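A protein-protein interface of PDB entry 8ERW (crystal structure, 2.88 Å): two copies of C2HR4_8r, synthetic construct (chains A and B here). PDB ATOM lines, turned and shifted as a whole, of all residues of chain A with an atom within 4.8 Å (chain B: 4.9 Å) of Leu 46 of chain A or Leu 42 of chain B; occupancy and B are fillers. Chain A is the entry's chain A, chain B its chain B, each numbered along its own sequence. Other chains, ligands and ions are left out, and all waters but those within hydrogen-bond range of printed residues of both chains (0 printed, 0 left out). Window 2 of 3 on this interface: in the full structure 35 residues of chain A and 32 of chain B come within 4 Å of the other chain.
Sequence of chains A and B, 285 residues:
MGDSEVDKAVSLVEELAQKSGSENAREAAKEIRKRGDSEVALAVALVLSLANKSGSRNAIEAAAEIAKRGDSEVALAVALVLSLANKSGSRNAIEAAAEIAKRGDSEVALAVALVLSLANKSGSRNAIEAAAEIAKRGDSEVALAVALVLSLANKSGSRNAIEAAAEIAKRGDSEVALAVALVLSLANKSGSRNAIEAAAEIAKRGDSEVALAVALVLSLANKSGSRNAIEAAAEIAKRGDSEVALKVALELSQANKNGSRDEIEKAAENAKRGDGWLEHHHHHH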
ATOM      1  N   LEU A  42       4.245  33.693  -1.723  1.00  0.00           N
ATOM      2  CA  LEU A  42       3.051  33.078  -2.294  1.00  0.00           C
ATOM      3  C   LEU A  42       3.269  31.590  -2.531  1.00  0.00           C
ATOM      4  O   LEU A  42       2.402  30.769  -2.205  1.00  0.00           O
ATOM      5  CB  LEU A  42       2.669  33.780  -3.596  1.00  0.00           C
ATOM      6  CG  LEU A  42       2.437  35.292  -3.548  1.00  0.00           C
ATOM      7  CD1 LEU A  42       1.696  35.749  -4.806  1.00  0.00           C
ATOM      8  CD2 LEU A  42       1.676  35.706  -2.305  1.00  0.00           C
ATOM      9  N   ALA A  43       4.426  31.225  -3.086  1.00  0.00           N
ATOM     10  CA  ALA A  43       4.753  29.820  -3.290  1.00  0.00           C
ATOM     11  C   ALA A  43       4.582  29.026  -2.001  1.00  0.00           C
ATOM     12  O   ALA A  43       3.839  28.039  -1.951  1.00  0.00           O
ATOM     13  CB  ALA A  43       6.186  29.693  -3.812  1.00  0.00           C
ATOM     14  N   VAL A  44       5.265  29.455  -0.939  1.00  0.00           N
ATOM     15  CA  VAL A  44       5.225  28.708   0.315  1.00  0.00           C
ATOM     16  C   VAL A  44       3.820  28.726   0.903  1.00  0.00           C
ATOM     17  O   VAL A  44       3.351  27.724   1.457  1.00  0.00           O
ATOM     18  CB  VAL A  44       6.260  29.268   1.306  1.00  0.00           C
ATOM     19  CG1 VAL A  44       6.070  28.638   2.672  1.00  0.00           C
ATOM     20  CG2 VAL A  44       7.659  29.023   0.781  1.00  0.00           C
ATOM     21  N   ALA A  45       3.134  29.866   0.808  1.00  0.00           N
ATOM     22  CA  ALA A  45       1.739  29.921   1.232  1.00  0.00           C
ATOM     23  C   ALA A  45       0.943  28.796   0.584  1.00  0.00           C
ATOM     24  O   ALA A  45       0.238  28.039   1.263  1.00  0.00           O
ATOM     25  CB  ALA A  45       1.138  31.283   0.880  1.00  0.00           C
ATOM     26  N   LEU A  46       1.058  28.665  -0.739  1.00  0.00           N
ATOM     27  CA  LEU A  46       0.387  27.574  -1.435  1.00  0.00           C
ATOM     28  C   LEU A  46       0.828  26.223  -0.891  1.00  0.00           C
ATOM     29  O   LEU A  46       0.001  25.323  -0.695  1.00  0.00           O
ATOM     30  CB  LEU A  46       0.667  27.661  -2.937  1.00  0.00           C
ATOM     31  N   VAL A  47       2.126  26.062  -0.632  1.00  0.00           N
ATOM     32  CA  VAL A  47       2.628  24.784  -0.139  1.00  0.00           C
ATOM     33  C   VAL A  47       1.982  24.445   1.199  1.00  0.00           C
ATOM     34  O   VAL A  47       1.511  23.323   1.416  1.00  0.00           O
ATOM     35  CB  VAL A  47       4.163  24.813  -0.029  1.00  0.00           C
ATOM     36  CG1 VAL A  47       4.669  23.527   0.608  1.00  0.00           C
ATOM     37  CG2 VAL A  47       4.789  25.013  -1.395  1.00  0.00           C
ATOM     38  N   LEU A  48       1.950  25.414   2.117  1.00  0.00           N
ATOM     39  CA  LEU A  48       1.379  25.153   3.434  1.00  0.00           C
ATOM     40  C   LEU A  48      -0.137  25.004   3.360  1.00  0.00           C
ATOM     41  O   LEU A  48      -0.712  24.123   4.011  1.00  0.00           O
ATOM     42  CB  LEU A  48       1.750  26.269   4.406  1.00  0.00           C
ATOM     43  CG  LEU A  48       3.191  26.291   4.907  1.00  0.00           C
ATOM     44  CD1 LEU A  48       3.336  27.338   6.006  1.00  0.00           C
ATOM     45  CD2 LEU A  48       3.631  24.928   5.410  1.00  0.00           C
ATOM     46  N   SER A  49      -0.802  25.864   2.587  1.00  0.00           N
ATOM     47  CA  SER A  49      -2.247  25.750   2.424  1.00  0.00           C
ATOM     48  C   SER A  49      -2.630  24.343   1.980  1.00  0.00           C
ATOM     49  O   SER A  49      -3.566  23.739   2.514  1.00  0.00           O
ATOM     50  CB  SER A  49      -2.744  26.791   1.419  1.00  0.00           C
ATOM     51  OG  SER A  49      -4.151  26.721   1.262  1.00  0.00           O
ATOM     52  N   LEU A  50      -1.902  23.802   1.000  1.00  0.00           N
ATOM     53  CA  LEU A  50      -2.177  22.445   0.541  1.00  0.00           C
ATOM     54  C   LEU A  50      -1.843  21.414   1.609  1.00  0.00           C
ATOM     55  O   LEU A  50      -2.474  20.353   1.663  1.00  0.00           O
ATOM     56  CB  LEU A  50      -1.389  22.162  -0.737  1.00  0.00           C
ATOM     57  CG  LEU A  50      -1.923  22.861  -1.988  1.00  0.00           C
ATOM     58  CD1 LEU A  50      -0.800  23.168  -2.963  1.00  0.00           C
ATOM     59  CD2 LEU A  50      -2.991  22.000  -2.655  1.00  0.00           C
ATOM     60  N   ALA A  79       4.233  21.972  -4.218  1.00  0.00           N
ATOM     61  CA  ALA A  79       2.816  22.306  -4.145  1.00  0.00           C
ATOM     62  C   ALA A  79       2.052  21.667  -5.297  1.00  0.00           C
ATOM     63  O   ALA A  79       0.950  21.137  -5.111  1.00  0.00           O
ATOM     64  CB  ALA A  79       2.632  23.824  -4.158  1.00  0.00           C
ATOM     65  N   ALA B   9      -6.945  35.458   0.419  1.00  0.00           N
ATOM     66  CA  ALA B   9      -6.305  35.106  -0.844  1.00  0.00           C
ATOM     67  C   ALA B   9      -6.920  35.874  -2.006  1.00  0.00           C
ATOM     68  O   ALA B   9      -6.204  36.347  -2.897  1.00  0.00           O
ATOM     69  CB  ALA B   9      -6.410  33.599  -1.083  1.00  0.00           C
ATOM     70  N   SER B  38      -9.238  28.669  -2.453  1.00  0.00           N
ATOM     71  CA  SER B  38      -7.959  29.236  -2.034  1.00  0.00           C
ATOM     72  C   SER B  38      -6.856  28.899  -3.031  1.00  0.00           C
ATOM     73  O   SER B  38      -6.185  29.793  -3.560  1.00  0.00           O
ATOM     74  CB  SER B  38      -7.597  28.724  -0.639  1.00  0.00           C
ATOM     75  OG  SER B  38      -8.693  28.849   0.247  1.00  0.00           O
ATOM     76  N   GLU B  39      -6.645  27.606  -3.290  1.00  0.00           N
ATOM     77  CA  GLU B  39      -5.567  27.185  -4.180  1.00  0.00           C
ATOM     78  C   GLU B  39      -5.600  27.967  -5.487  1.00  0.00           C
ATOM     79  O   GLU B  39      -4.606  28.581  -5.888  1.00  0.00           O
ATOM     80  CB  GLU B  39      -5.667  25.681  -4.454  1.00  0.00           C
ATOM     81  CG  GLU B  39      -4.753  25.204  -5.574  1.00  0.00           C
ATOM     82  CD  GLU B  39      -4.775  23.698  -5.758  1.00  0.00           C
ATOM     83  OE1 GLU B  39      -5.283  22.990  -4.863  1.00  0.00           O
ATOM     84  OE2 GLU B  39      -4.282  23.220  -6.804  1.00  0.00           O
ATOM     85  N   VAL B  40      -6.746  27.941  -6.173  1.00  0.00           N
ATOM     86  CA  VAL B  40      -6.891  28.720  -7.398  1.00  0.00           C
ATOM     87  C   VAL B  40      -6.538  30.175  -7.137  1.00  0.00           C
ATOM     88  O   VAL B  40      -5.820  30.810  -7.920  1.00  0.00           O
ATOM     89  CB  VAL B  40      -8.322  28.577  -7.953  1.00  0.00           C
ATOM     90  CG1 VAL B  40      -8.474  29.380  -9.235  1.00  0.00           C
ATOM     91  CG2 VAL B  40      -8.662  27.113  -8.184  1.00  0.00           C
ATOM     92  N   ALA B  41      -7.026  30.722  -6.023  1.00  0.00           N
ATOM     93  CA  ALA B  41      -6.758  32.117  -5.693  1.00  0.00           C
ATOM     94  C   ALA B  41      -5.260  32.370  -5.580  1.00  0.00           C
ATOM     95  O   ALA B  41      -4.704  33.230  -6.273  1.00  0.00           O
ATOM     96  CB  ALA B  41      -7.468  32.491  -4.390  1.00  0.00           C
ATOM     97  N   LEU B  42      -4.589  31.630  -4.694  1.00  0.00           N
ATOM     98  CA  LEU B  42      -3.140  31.753  -4.578  1.00  0.00           C
ATOM     99  C   LEU B  42      -2.465  31.428  -5.905  1.00  0.00           C
ATOM    100  O   LEU B  42      -1.613  32.185  -6.386  1.00  0.00           O
ATOM    101  CB  LEU B  42      -2.623  30.830  -3.476  1.00  0.00           C
ATOM    102  CG  LEU B  42      -3.131  31.086  -2.057  1.00  0.00           C
ATOM    103  CD1 LEU B  42      -2.549  30.066  -1.088  1.00  0.00           C
ATOM    104  CD2 LEU B  42      -2.790  32.497  -1.616  1.00  0.00           C
ATOM    105  N   ALA B  43      -2.844  30.302  -6.513  1.00  0.00           N
ATOM    106  CA  ALA B  43      -2.263  29.905  -7.790  1.00  0.00           C
ATOM    107  C   ALA B  43      -2.297  31.052  -8.790  1.00  0.00           C
ATOM    108  O   ALA B  43      -1.305  31.331  -9.472  1.00  0.00           O
ATOM    109  CB  ALA B  43      -3.006  28.689  -8.345  1.00  0.00           C
ATOM    110  N   VAL B  44      -3.436  31.739  -8.885  1.00  0.00           N
ATOM    111  CA  VAL B  44      -3.556  32.819  -9.856  1.00  0.00           C
ATOM    112  C   VAL B  44      -2.745  34.029  -9.414  1.00  0.00           C
ATOM    113  O   VAL B  44      -2.109  34.700 -10.237  1.00  0.00           O
ATOM    114  CB  VAL B  44      -5.036  33.183 -10.076  1.00  0.00           C
ATOM    115  CG1 VAL B  44      -5.144  34.480 -10.857  1.00  0.00           C
ATOM    116  CG2 VAL B  44      -5.741  32.052 -10.795  1.00  0.00           C
ATOM    117  N   ALA B  45      -2.770  34.343  -8.116  1.00  0.00           N
ATOM    118  CA  ALA B  45      -1.934  35.421  -7.603  1.00  0.00           C
ATOM    119  C   ALA B  45      -0.504  35.260  -8.101  1.00  0.00           C
ATOM    120  O   ALA B  45       0.127  36.221  -8.556  1.00  0.00           O
ATOM    121  CB  ALA B  45      -1.976  35.440  -6.076  1.00  0.00           C
ATOM    122  N   LEU B  46       0.018  34.034  -8.028  1.00  0.00           N
ATOM    123  CA  LEU B  46       1.322  33.744  -8.612  1.00  0.00           C
ATOM    124  C   LEU B  46       1.353  34.123 -10.086  1.00  0.00           C
ATOM    125  O   LEU B  46       2.248  34.848 -10.537  1.00  0.00           O
ATOM    126  CB  LEU B  46       1.649  32.261  -8.443  1.00  0.00           C
ATOM    127  CG  LEU B  46       1.837  31.743  -7.021  1.00  0.00           C
ATOM    128  CD1 LEU B  46       1.842  30.225  -6.992  1.00  0.00           C
ATOM    129  CD2 LEU B  46       3.130  32.289  -6.444  1.00  0.00           C
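Leu 46 of chain A touches one residue of chain B.
Of the printed residues of chain B, Leu 50 of chain A touches Glu 39 (3.3 Å).
Ser 38 of chain B touches none of the printed residues of chain A.
Val 40 of chain B touches none of the printed residues of chain A.
Leu 42 of chain B touches just one residue of chain A: Leu 46.
Printed residues of chain A within 4 Å of Ala 45 of chain B: Leu 42.
Printed residues of chain A within 4 Å of Leu 46 of chain B: Leu 42 and Ala 43.
The nearest printed residue of chain B that does not touch Leu 46 of chain A is Leu 46 of chain B (4.9 Å).
The nearest printed residue of chain B that does not touch Ala 43 of chain A is Leu 42 of chain B (6.8 Å).
Leu 42 of chain A touches Ala 45 of chain B, but with the chains exchanged Ala 45 of chain A does not touch Leu 42 of chain B (4.1 Å).
Leu 42 of chain A touches Leu 46 of chain B, and with the chains exchanged Leu 46 of chain A touches Leu 42 of chain B.
Ala 43 of chain A touches Leu 46 of chain B, but with the chains exchanged Leu 46 of chain A does not touch Ala 43 of chain B (5.7 Å).
Of the 5 pairs that touch across the chains among the printed residues, 2 have their exchanged pair printed and touching as well.
Hydrophobic or aromatic side chains of chain A within 4 Å of the printed part of chain B: Leu 42 and Leu 50.
Among the printed residues, 5 pairs touch across the chains.
Among the printed residues, pairs that only touch across the chains: Leu 42 of chain A with Ala 45 of chain B (3.9 Å), Leu 42 of chain A with Leu 46 of chain B (3.2 Å), Ala 43 of chain A with Leu 46 of chain B (3.8 Å), Leu 46 of chain A with Leu 42 of chain B (3.9 Å) and Leu 50 of chain A with Glu 39 of chain B (3.3 Å).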
